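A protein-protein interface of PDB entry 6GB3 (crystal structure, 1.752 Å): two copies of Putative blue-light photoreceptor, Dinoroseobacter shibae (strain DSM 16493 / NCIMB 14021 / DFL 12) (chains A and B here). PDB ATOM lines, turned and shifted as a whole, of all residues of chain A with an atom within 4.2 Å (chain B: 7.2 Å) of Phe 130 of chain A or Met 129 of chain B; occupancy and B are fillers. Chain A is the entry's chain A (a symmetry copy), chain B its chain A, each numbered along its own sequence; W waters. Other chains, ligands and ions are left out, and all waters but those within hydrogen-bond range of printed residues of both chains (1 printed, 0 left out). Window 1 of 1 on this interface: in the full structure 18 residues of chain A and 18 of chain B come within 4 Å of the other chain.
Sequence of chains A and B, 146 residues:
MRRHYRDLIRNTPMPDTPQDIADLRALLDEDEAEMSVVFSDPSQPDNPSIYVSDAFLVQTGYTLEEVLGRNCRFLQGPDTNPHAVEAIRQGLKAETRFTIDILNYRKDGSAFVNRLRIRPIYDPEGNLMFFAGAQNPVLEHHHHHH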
ATOM      1  N   ALA A  22      17.301   8.479  -4.744  1.00  0.00           N
ATOM      2  CA  ALA A  22      15.903   8.811  -4.526  1.00  0.00           C
ATOM      3  C   ALA A  22      15.771  10.142  -3.793  1.00  0.00           C
ATOM      4  O   ALA A  22      16.465  10.393  -2.803  1.00  0.00           O
ATOM      5  CB  ALA A  22      15.221   7.696  -3.732  1.00  0.00           C
ATOM      6  N   LEU A  24      13.932  11.439  -1.416  1.00  0.00           N
ATOM      7  CA  LEU A  24      13.009  11.086  -0.343  1.00  0.00           C
ATOM      8  C   LEU A  24      12.240  12.302   0.151  1.00  0.00           C
ATOM      9  O   LEU A  24      11.067  12.187   0.524  1.00  0.00           O
ATOM     10  CB  LEU A  24      13.761  10.426   0.811  1.00  0.00           C
ATOM     11  CG  LEU A  24      14.494   9.142   0.421  1.00  0.00           C
ATOM     12  CD1 LEU A  24      14.990   8.397   1.641  1.00  0.00           C
ATOM     13  CD2 LEU A  24      13.592   8.255  -0.417  1.00  0.00           C
ATOM     14  N   SER A  40      12.173   6.479   8.004  1.00  0.00           N
ATOM     15  CA  SER A  40      12.701   5.173   8.365  1.00  0.00           C
ATOM     16  C   SER A  40      12.155   4.115   7.417  1.00  0.00           C
ATOM     17  O   SER A  40      11.131   4.310   6.751  1.00  0.00           O
ATOM     18  CB  SER A  40      12.344   4.799   9.808  1.00  0.00           C
ATOM     19  OG  SER A  40      10.979   4.399   9.898  1.00  0.00           O
ATOM     20  N   PRO A  42      10.852   0.464   7.706  1.00  0.00           N
ATOM     21  CA  PRO A  42      10.457  -0.628   8.613  1.00  0.00           C
ATOM     22  C   PRO A  42      10.683  -2.021   8.046  1.00  0.00           C
ATOM     23  O   PRO A  42      10.588  -2.995   8.801  1.00  0.00           O
ATOM     24  CB  PRO A  42       8.964  -0.364   8.849  1.00  0.00           C
ATOM     25  CG  PRO A  42       8.524   0.439   7.654  1.00  0.00           C
ATOM     26  CD  PRO A  42       9.706   1.253   7.224  1.00  0.00           C
ATOM     27  N   ILE A  50      16.579   6.149   6.965  1.00  0.00           N
ATOM     28  CA  ILE A  50      17.152   6.190   5.621  1.00  0.00           C
ATOM     29  C   ILE A  50      17.319   7.604   5.112  1.00  0.00           C
ATOM     30  O   ILE A  50      18.015   7.804   4.103  1.00  0.00           O
ATOM     31  CB  ILE A  50      16.319   5.370   4.614  1.00  0.00           C
ATOM     32  CG1 ILE A  50      14.910   5.959   4.479  1.00  0.00           C
ATOM     33  CG2 ILE A  50      16.304   3.898   5.015  1.00  0.00           C
ATOM     34  CD1 ILE A  50      14.065   5.297   3.415  1.00  0.00           C
ATOM     35  N   PRO A 120       2.610   6.842   9.092  1.00  0.00           N
ATOM     36  CA  PRO A 120       3.022   5.802   8.149  1.00  0.00           C
ATOM     37  C   PRO A 120       2.833   6.268   6.712  1.00  0.00           C
ATOM     38  O   PRO A 120       1.983   7.109   6.412  1.00  0.00           O
ATOM     39  CB  PRO A 120       2.077   4.644   8.482  1.00  0.00           C
ATOM     40  CG  PRO A 120       0.818   5.342   8.890  1.00  0.00           C
ATOM     41  CD  PRO A 120       1.249   6.610   9.607  1.00  0.00           C
ATOM     42  N   ILE A 121       3.647   5.704   5.822  1.00  0.00           N
ATOM     43  CA  ILE A 121       3.560   5.961   4.390  1.00  0.00           C
ATOM     44  C   ILE A 121       3.471   4.615   3.680  1.00  0.00           C
ATOM     45  O   ILE A 121       4.274   3.718   3.954  1.00  0.00           O
ATOM     46  CB  ILE A 121       4.770   6.772   3.880  1.00  0.00           C
ATOM     47  CG1 ILE A 121       4.896   8.088   4.648  1.00  0.00           C
ATOM     48  CG2 ILE A 121       4.639   7.052   2.389  1.00  0.00           C
ATOM     49  CD1 ILE A 121       6.159   8.849   4.332  1.00  0.00           C
ATOM     50  N   LEU A 128       2.765  -1.130   4.034  1.00  0.00           N
ATOM     51  CA  LEU A 128       3.588  -0.142   4.715  1.00  0.00           C
ATOM     52  C   LEU A 128       4.952  -0.057   4.046  1.00  0.00           C
ATOM     53  O   LEU A 128       5.580  -1.077   3.745  1.00  0.00           O
ATOM     54  CB  LEU A 128       3.735  -0.497   6.190  1.00  0.00           C
ATOM     55  CG  LEU A 128       4.615   0.453   7.006  1.00  0.00           C
ATOM     56  CD1 LEU A 128       4.001   1.846   7.073  1.00  0.00           C
ATOM     57  CD2 LEU A 128       4.842  -0.110   8.393  1.00  0.00           C
ATOM     58  N   MET A 129       5.399   1.167   3.797  1.00  0.00           N
ATOM     59  CA  MET A 129       6.625   1.420   3.055  1.00  0.00           C
ATOM     60  C   MET A 129       7.657   2.170   3.881  1.00  0.00           C
ATOM     61  O   MET A 129       8.823   1.764   3.933  1.00  0.00           O
ATOM     62  CB  MET A 129       6.287   2.213   1.789  1.00  0.00           C
ATOM     63  CG  MET A 129       7.310   2.110   0.697  1.00  0.00           C
ATOM     64  SD  MET A 129       6.756   3.025  -0.750  1.00  0.00           S
ATOM     65  CE  MET A 129       8.116   2.690  -1.867  1.00  0.00           C
ATOM     66  N   PHE A 130       7.251   3.263   4.522  1.00  0.00           N
ATOM     67  CA  PHE A 130       8.137   4.100   5.316  1.00  0.00           C
ATOM     68  C   PHE A 130       7.369   4.618   6.518  1.00  0.00           C
ATOM     69  O   PHE A 130       6.137   4.605   6.545  1.00  0.00           O
ATOM     70  CB  PHE A 130       8.663   5.311   4.528  1.00  0.00           C
ATOM     71  CG  PHE A 130       9.281   4.970   3.208  1.00  0.00           C
ATOM     72  CD1 PHE A 130      10.547   4.419   3.148  1.00  0.00           C
ATOM     73  CD2 PHE A 130       8.610   5.235   2.022  1.00  0.00           C
ATOM     74  CE1 PHE A 130      11.126   4.116   1.931  1.00  0.00           C
ATOM     75  CE2 PHE A 130       9.190   4.938   0.802  1.00  0.00           C
ATOM     76  CZ  PHE A 130      10.445   4.375   0.757  1.00  0.00           C
ATOM     77  N   PHE A 131       8.116   5.102   7.507  1.00  0.00           N
ATOM     78  CA  PHE A 131       7.579   5.999   8.518  1.00  0.00           C
ATOM     79  C   PHE A 131       8.214   7.373   8.326  1.00  0.00           C
ATOM     80  O   PHE A 131       9.390   7.478   7.953  1.00  0.00           O
ATOM     81  CB  PHE A 131       7.860   5.491   9.940  1.00  0.00           C
ATOM     82  CG  PHE A 131       6.999   4.326  10.362  1.00  0.00           C
ATOM     83  CD1 PHE A 131       5.654   4.506  10.662  1.00  0.00           C
ATOM     84  CD2 PHE A 131       7.543   3.061  10.493  1.00  0.00           C
ATOM     85  CE1 PHE A 131       4.856   3.432  11.056  1.00  0.00           C
ATOM     86  CE2 PHE A 131       6.757   1.984  10.897  1.00  0.00           C
ATOM     87  CZ  PHE A 131       5.413   2.170  11.180  1.00  0.00           C
ATOM     88  N   ASP B  20      -1.692   7.504   3.806  1.00  0.00           N
ATOM     89  CA  ASP B  20      -0.995   8.352   2.845  1.00  0.00           C
ATOM     90  C   ASP B  20      -0.078   7.513   1.954  1.00  0.00           C
ATOM     91  O   ASP B  20       0.621   6.620   2.435  1.00  0.00           O
ATOM     92  CB  ASP B  20      -0.192   9.430   3.570  1.00  0.00           C
ATOM     93  CG  ASP B  20      -0.196  10.751   2.830  1.00  0.00           C
ATOM     94  OD1 ASP B  20      -1.169  11.011   2.088  1.00  0.00           O
ATOM     95  OD2 ASP B  20       0.770  11.528   2.989  1.00  0.00           O
ATOM     96  N   ALA B  22       2.935   6.993  -0.938  1.00  0.00           N
ATOM     97  CA  ALA B  22       4.141   7.538  -1.539  1.00  0.00           C
ATOM     98  C   ALA B  22       3.905   7.889  -3.004  1.00  0.00           C
ATOM     99  O   ALA B  22       3.328   7.102  -3.760  1.00  0.00           O
ATOM    100  CB  ALA B  22       5.287   6.534  -1.409  1.00  0.00           C
ATOM    101  N   LEU B  24       5.509   7.664  -5.849  1.00  0.00           N
ATOM    102  CA  LEU B  24       6.651   7.018  -6.486  1.00  0.00           C
ATOM    103  C   LEU B  24       7.006   7.691  -7.803  1.00  0.00           C
ATOM    104  O   LEU B  24       8.187   7.774  -8.162  1.00  0.00           O
ATOM    105  CB  LEU B  24       6.368   5.533  -6.706  1.00  0.00           C
ATOM    106  CG  LEU B  24       6.085   4.758  -5.419  1.00  0.00           C
ATOM    107  CD1 LEU B  24       6.079   3.265  -5.664  1.00  0.00           C
ATOM    108  CD2 LEU B  24       7.102   5.121  -4.352  1.00  0.00           C
ATOM    109  N   SER B  40      10.337  -1.400  -9.159  1.00  0.00           N
ATOM    110  CA  SER B  40      10.367  -2.645  -8.409  1.00  0.00           C
ATOM    111  C   SER B  40      11.099  -2.436  -7.090  1.00  0.00           C
ATOM    112  O   SER B  40      11.872  -1.485  -6.924  1.00  0.00           O
ATOM    113  CB  SER B  40      11.050  -3.765  -9.201  1.00  0.00           C
ATOM    114  OG  SER B  40      12.465  -3.592  -9.192  1.00  0.00           O
ATOM    115  N   ASP B  41      10.852  -3.350  -6.158  1.00  0.00           N
ATOM    116  CA  ASP B  41      11.458  -3.309  -4.829  1.00  0.00           C
ATOM    117  C   ASP B  41      12.329  -4.542  -4.671  1.00  0.00           C
ATOM    118  O   ASP B  41      11.827  -5.621  -4.303  1.00  0.00           O
ATOM    119  CB  ASP B  41      10.394  -3.257  -3.732  1.00  0.00           C
ATOM    120  CG  ASP B  41      10.994  -3.057  -2.346  1.00  0.00           C
ATOM    121  OD1 ASP B  41      12.238  -3.059  -2.219  1.00  0.00           O
ATOM    122  OD2 ASP B  41      10.215  -2.904  -1.380  1.00  0.00           O
ATOM    123  N   PRO B  42      13.636  -4.428  -4.921  1.00  0.00           N
ATOM    124  CA  PRO B  42      14.526  -5.599  -4.843  1.00  0.00           C
ATOM    125  C   PRO B  42      14.723  -6.138  -3.434  1.00  0.00           C
ATOM    126  O   PRO B  42      15.271  -7.236  -3.287  1.00  0.00           O
ATOM    127  CB  PRO B  42      15.847  -5.075  -5.422  1.00  0.00           C
ATOM    128  CG  PRO B  42      15.785  -3.583  -5.227  1.00  0.00           C
ATOM    129  CD  PRO B  42      14.341  -3.197  -5.319  1.00  0.00           C
ATOM    130  N   SER B  43      14.303  -5.410  -2.404  1.00  0.00           N
ATOM    131  CA  SER B  43      14.375  -5.926  -1.046  1.00  0.00           C
ATOM    132  C   SER B  43      13.198  -6.831  -0.702  1.00  0.00           C
ATOM    133  O   SER B  43      13.200  -7.449   0.362  1.00  0.00           O
ATOM    134  CB  SER B  43      14.455  -4.767  -0.052  1.00  0.00           C
ATOM    135  OG  SER B  43      13.198  -4.124   0.088  1.00  0.00           O
ATOM    136  N   ASN B  47      11.666  -9.493  -6.215  1.00  0.00           N
ATOM    137  CA  ASN B  47      11.797  -8.175  -6.833  1.00  0.00           C
ATOM    138  C   ASN B  47      10.496  -7.719  -7.505  1.00  0.00           C
ATOM    139  O   ASN B  47      10.468  -7.460  -8.715  1.00  0.00           O
ATOM    140  CB  ASN B  47      12.951  -8.181  -7.826  1.00  0.00           C
ATOM    141  CG  ASN B  47      13.359  -6.792  -8.294  1.00  0.00           C
ATOM    142  OD1 ASN B  47      13.063  -5.781  -7.651  1.00  0.00           O
ATOM    143  ND2 ASN B  47      14.055  -6.740  -9.421  1.00  0.00           N
ATOM    144  N   ILE B  50       6.228  -2.430  -7.528  1.00  0.00           N
ATOM    145  CA  ILE B  50       5.478  -1.661  -6.536  1.00  0.00           C
ATOM    146  C   ILE B  50       4.746  -0.490  -7.153  1.00  0.00           C
ATOM    147  O   ILE B  50       3.877   0.097  -6.488  1.00  0.00           O
ATOM    148  CB  ILE B  50       6.382  -1.163  -5.389  1.00  0.00           C
ATOM    149  CG1 ILE B  50       7.453  -0.206  -5.927  1.00  0.00           C
ATOM    150  CG2 ILE B  50       6.978  -2.346  -4.634  1.00  0.00           C
ATOM    151  CD1 ILE B  50       8.302   0.433  -4.854  1.00  0.00           C
ATOM    152  N   GLU B  95      23.740  -3.894 -10.952  1.00  0.00           N
ATOM    153  CA  GLU B  95      23.280  -2.586 -10.487  1.00  0.00           C
ATOM    154  C   GLU B  95      23.866  -1.469 -11.350  1.00  0.00           C
ATOM    155  O   GLU B  95      24.582  -0.579 -10.889  1.00  0.00           O
ATOM    156  CB  GLU B  95      23.610  -2.388  -9.007  1.00  0.00           C
ATOM    157  CG  GLU B  95      22.864  -3.346  -8.110  1.00  0.00           C
ATOM    158  CD  GLU B  95      23.179  -3.159  -6.642  1.00  0.00           C
ATOM    159  OE1 GLU B  95      23.599  -2.050  -6.245  1.00  0.00           O
ATOM    160  OE2 GLU B  95      23.001  -4.133  -5.884  1.00  0.00           O
ATOM    161  N   PRO B 120      19.199   1.439 -11.642  1.00  0.00           N
ATOM    162  CA  PRO B 120      19.042   1.317 -10.192  1.00  0.00           C
ATOM    163  C   PRO B 120      18.830   2.682  -9.553  1.00  0.00           C
ATOM    164  O   PRO B 120      19.270   3.712 -10.068  1.00  0.00           O
ATOM    165  CB  PRO B 120      20.374   0.703  -9.754  1.00  0.00           C
ATOM    166  CG  PRO B 120      21.352   1.291 -10.722  1.00  0.00           C
ATOM    167  CD  PRO B 120      20.616   1.415 -12.045  1.00  0.00           C
ATOM    168  N   ILE B 121      18.141   2.674  -8.414  1.00  0.00           N
ATOM    169  CA  ILE B 121      17.910   3.871  -7.616  1.00  0.00           C
ATOM    170  C   ILE B 121      18.359   3.573  -6.189  1.00  0.00           C
ATOM    171  O   ILE B 121      17.977   2.544  -5.624  1.00  0.00           O
ATOM    172  CB  ILE B 121      16.428   4.301  -7.646  1.00  0.00           C
ATOM    173  CG1 ILE B 121      15.964   4.527  -9.086  1.00  0.00           C
ATOM    174  CG2 ILE B 121      16.220   5.570  -6.830  1.00  0.00           C
ATOM    175  CD1 ILE B 121      14.481   4.771  -9.208  1.00  0.00           C
ATOM    176  N   TYR B 122      19.169   4.465  -5.609  1.00  0.00           N
ATOM    177  CA  TYR B 122      19.765   4.250  -4.294  1.00  0.00           C
ATOM    178  C   TYR B 122      19.160   5.186  -3.252  1.00  0.00           C
ATOM    179  O   TYR B 122      18.576   6.222  -3.583  1.00  0.00           O
ATOM    180  CB  TYR B 122      21.289   4.448  -4.349  1.00  0.00           C
ATOM    181  CG  TYR B 122      21.974   3.484  -5.292  1.00  0.00           C
ATOM    182  CD1 TYR B 122      22.382   2.231  -4.854  1.00  0.00           C
ATOM    183  CD2 TYR B 122      22.195   3.818  -6.625  1.00  0.00           C
ATOM    184  CE1 TYR B 122      22.993   1.339  -5.711  1.00  0.00           C
ATOM    185  CE2 TYR B 122      22.808   2.934  -7.490  1.00  0.00           C
ATOM    186  CZ  TYR B 122      23.205   1.695  -7.029  1.00  0.00           C
ATOM    187  OH  TYR B 122      23.817   0.806  -7.881  1.00  0.00           O
ATOM    188  N   ASP B 123      19.302   4.807  -1.984  1.00  0.00           N
ATOM    189  CA  ASP B 123      18.930   5.677  -0.873  1.00  0.00           C
ATOM    190  C   ASP B 123      20.126   6.531  -0.468  1.00  0.00           C
ATOM    191  O   ASP B 123      21.251   6.285  -0.911  1.00  0.00           O
ATOM    192  CB  ASP B 123      18.368   4.846   0.293  1.00  0.00           C
ATOM    193  CG  ASP B 123      19.379   3.875   0.914  1.00  0.00           C
ATOM    194  OD1 ASP B 123      20.602   4.094   0.821  1.00  0.00           O
ATOM    195  OD2 ASP B 123      18.926   2.884   1.537  1.00  0.00           O
ATOM    196  N   PRO B 124      19.908   7.578   0.347  1.00  0.00           N
ATOM    197  CA  PRO B 124      21.028   8.453   0.740  1.00  0.00           C
ATOM    198  C   PRO B 124      22.236   7.725   1.312  1.00  0.00           C
ATOM    199  O   PRO B 124      23.365   8.223   1.194  1.00  0.00           O
ATOM    200  CB  PRO B 124      20.385   9.372   1.790  1.00  0.00           C
ATOM    201  CG  PRO B 124      18.977   9.497   1.331  1.00  0.00           C
ATOM    202  CD  PRO B 124      18.608   8.147   0.756  1.00  0.00           C
ATOM    203  N   GLY B 126      23.376   5.025   0.130  1.00  0.00           N
ATOM    204  CA  GLY B 126      24.014   4.351  -0.975  1.00  0.00           C
ATOM    205  C   GLY B 126      23.605   2.910  -1.143  1.00  0.00           C
ATOM    206  O   GLY B 126      24.224   2.205  -1.945  1.00  0.00           O
ATOM    207  N   ASN B 127      22.608   2.446  -0.393  1.00  0.00           N
ATOM    208  CA  ASN B 127      22.079   1.107  -0.569  1.00  0.00           C
ATOM    209  C   ASN B 127      21.082   1.109  -1.718  1.00  0.00           C
ATOM    210  O   ASN B 127      20.324   2.068  -1.900  1.00  0.00           O
ATOM    211  CB  ASN B 127      21.388   0.619   0.707  1.00  0.00           C
ATOM    212  CG  ASN B 127      22.310   0.595   1.902  1.00  0.00           C
ATOM    213  OD1 ASN B 127      23.530   0.507   1.760  1.00  0.00           O
ATOM    214  ND2 ASN B 127      21.727   0.667   3.096  1.00  0.00           N
ATOM    215  N   LEU B 128      21.095   0.035  -2.499  1.00  0.00           N
ATOM    216  CA  LEU B 128      20.092  -0.127  -3.540  1.00  0.00           C
ATOM    217  C   LEU B 128      18.700  -0.086  -2.926  1.00  0.00           C
ATOM    218  O   LEU B 128      18.435  -0.724  -1.902  1.00  0.00           O
ATOM    219  CB  LEU B 128      20.309  -1.437  -4.290  1.00  0.00           C
ATOM    220  CG  LEU B 128      19.287  -1.737  -5.389  1.00  0.00           C
ATOM    221  CD1 LEU B 128      19.371  -0.709  -6.511  1.00  0.00           C
ATOM    222  CD2 LEU B 128      19.490  -3.140  -5.919  1.00  0.00           C
ATOM    223  N   MET B 129      17.816   0.685  -3.546  1.00  0.00           N
ATOM    224  CA  MET B 129      16.481   0.930  -3.021  1.00  0.00           C
ATOM    225  C   MET B 129      15.392   0.446  -3.963  1.00  0.00           C
ATOM    226  O   MET B 129      14.468  -0.253  -3.533  1.00  0.00           O
ATOM    227  CB  MET B 129      16.318   2.429  -2.753  1.00  0.00           C
ATOM    228  CG  MET B 129      15.242   2.773  -1.767  1.00  0.00           C
ATOM    229  SD  MET B 129      15.207   4.551  -1.492  1.00  0.00           S
ATOM    230  CE  MET B 129      13.899   4.649  -0.273  1.00  0.00           C
ATOM    231  N   PHE B 130      15.479   0.811  -5.239  1.00  0.00           N
ATOM    232  CA  PHE B 130      14.488   0.454  -6.242  1.00  0.00           C
ATOM    233  C   PHE B 130      15.198   0.199  -7.559  1.00  0.00           C
ATOM    234  O   PHE B 130      16.344   0.607  -7.758  1.00  0.00           O
ATOM    235  CB  PHE B 130      13.453   1.569  -6.467  1.00  0.00           C
ATOM    236  CG  PHE B 130      12.800   2.069  -5.217  1.00  0.00           C
ATOM    237  CD1 PHE B 130      11.817   1.325  -4.592  1.00  0.00           C
ATOM    238  CD2 PHE B 130      13.142   3.305  -4.685  1.00  0.00           C
ATOM    239  CE1 PHE B 130      11.203   1.790  -3.447  1.00  0.00           C
ATOM    240  CE2 PHE B 130      12.525   3.776  -3.540  1.00  0.00           C
ATOM    241  CZ  PHE B 130      11.559   3.016  -2.920  1.00  0.00           C
ATOM    242  N   PHE B 131      14.490  -0.463  -8.470  1.00  0.00           N
ATOM    243  CA  PHE B 131      14.824  -0.433  -9.885  1.00  0.00           C
ATOM    244  C   PHE B 131      13.723   0.324 -10.621  1.00  0.00           C
ATOM    245  O   PHE B 131      12.544   0.235 -10.256  1.00  0.00           O
ATOM    246  CB  PHE B 131      14.964  -1.846 -10.470  1.00  0.00           C
ATOM    247  CG  PHE B 131      16.235  -2.556 -10.075  1.00  0.00           C
ATOM    248  CD1 PHE B 131      17.458  -2.181 -10.617  1.00  0.00           C
ATOM    249  CD2 PHE B 131      16.200  -3.620  -9.192  1.00  0.00           C
ATOM    250  CE1 PHE B 131      18.635  -2.838 -10.257  1.00  0.00           C
ATOM    251  CE2 PHE B 131      17.368  -4.290  -8.835  1.00  0.00           C
ATOM    252  CZ  PHE B 131      18.586  -3.900  -9.369  1.00  0.00           C
HETATM  253  O   HOH W   1      19.652   5.872   3.432  1.00  0.00           O
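O of Tyr 122 of chain B sits at hydrogen-bond distance from N of Ala 22 of chain A, at 2.8 Å.
Water W1 lies within hydrogen-bond range of O of Ile 50 of chain A and OD1 of Asp 123 of chain B.
Of the printed residues of chain B, Ala 22 of chain A touches Ile 121 (3.7 Å), Tyr 122 (2.8 Å) and Met 129 (3.9 Å). Printed residues of chain B within 4 Å of Phe 130 of chain A: Met 129 (3.6 Å). Printed residues of chain A within 4 Å of Leu 24 of chain B: Met 129. Printed residues of chain A within 4 Å of Ile 50 of chain B: Met 129 (3.7 Å). Leu 128 of chain B touches none of the printed residues of chain A. Met 129 of chain B touches just these residues of chain A: Ala 22 (3.9 Å), Leu 24 (3.6 Å), Ile 50 (3.7 Å) and Phe 130 (3.6 Å). Of the printed residues of chain A, Phe 130 of chain B touches Met 129. The nearest residue of chain B that does not touch Phe 130 of chain A is Phe 130 of chain B (4.1 Å). The nearest printed residue of chain A that does not touch Met 129 of chain B is Met 129 of chain A (6.3 Å).
Among the printed residues, merely in contact across the chains: Ala 22 of chain A with Ile 121 of chain B (3.7 Å), Ala 22 of chain A with Met 129 of chain B (3.9 Å), Leu 24 of chain A with Pro 124 of chain B (3.7 Å), Leu 24 of chain A with Met 129 of chain B (3.6 Å), Ile 50 of chain A with Pro 124 of chain B (3.4 Å), Ile 50 of chain A with Met 129 of chain B (3.7 Å), Ile 121 of chain A with Asp 20 of chain B (3.6 Å), Ile 121 of chain A with Ala 22 of chain B (3.7 Å), Met 129 of chain A with Ala 22 of chain B (3.9 Å), Met 129 of chain A with Leu 24 of chain B (3.6 Å), Met 129 of chain A with Ile 50 of chain B (3.7 Å), Met 129 of chain A with Phe 130 of chain B (3.6 Å) and Phe 130 of chain A with Met 129 of chain B (3.6 Å).
Ala 22 of chain A touches Ile 121 of chain B, and with the chains exchanged Ile 121 of chain A touches Ala 22 of chain B. Ala 22 of chain A touches Met 129 of chain B, and with the chains exchanged Met 129 of chain A touches Ala 22 of chain B. Leu 24 of chain A touches Met 129 of chain B, and with the chains exchanged Met 129 of chain A touches Leu 24 of chain B. Ile 50 of chain A touches Met 129 of chain B, and with the chains exchanged Met 129 of chain A touches Ile 50 of chain B. Of the 14 pairs that touch across the chains among the printed residues, 10 have their exchanged pair printed and touching as well.
Printed residues of chain B that touch a printed residue of chain A: Asp 20, Ala 22, Leu 24, Ile 50, Ile 121, Tyr 122, Pro 124, Met 129 and Phe 130. Hydrophobic or aromatic side chains of chain B that line the printed part of chain A: Ala 22, Leu 24, Ile 50, Ile 121, Pro 124, Met 129 and Phe 130. Of the 11 printed residues of chain A, 6 touch a printed residue of chain B. Printed residues of chain A that touch a printed residue of chain B: Ala 22, Leu 24, Ile 50, Ile 121, Met 129 and Phe 130. Hydrophobic or aromatic side chains of chain A within 4 Å of the printed part of chain B: Ala 22, Leu 24, Ile 50, Ile 121, Met 129 and Phe 130.
The backbone NH (N) of Ile 121 of chain B is in hydrogen-bond range of the backbone carbonyl oxygen (O) of Phe 130 of chain B, at 2.8 Å. N of Ile 121 of chain A lies within hydrogen-bond range of O of Phe 130 of chain A, 2.8 Å away. The backbone carbonyl oxygen (O) of Ile 121 of chain B is in hydrogen-bond range of the backbone NH (N) of Met 129 of chain B (2.8 Å). The side-chain hydroxyl (OH) of Tyr 122 of chain B sits at hydrogen-bond distance from the side-chain carboxylate (OE1) of Glu 95 of chain B (3.3 Å). The backbone carbonyl oxygen (O) of Ile 121 of chain A is in hydrogen-bond range of the backbone NH (N) of Met 129 of chain A, at 2.8 Å.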
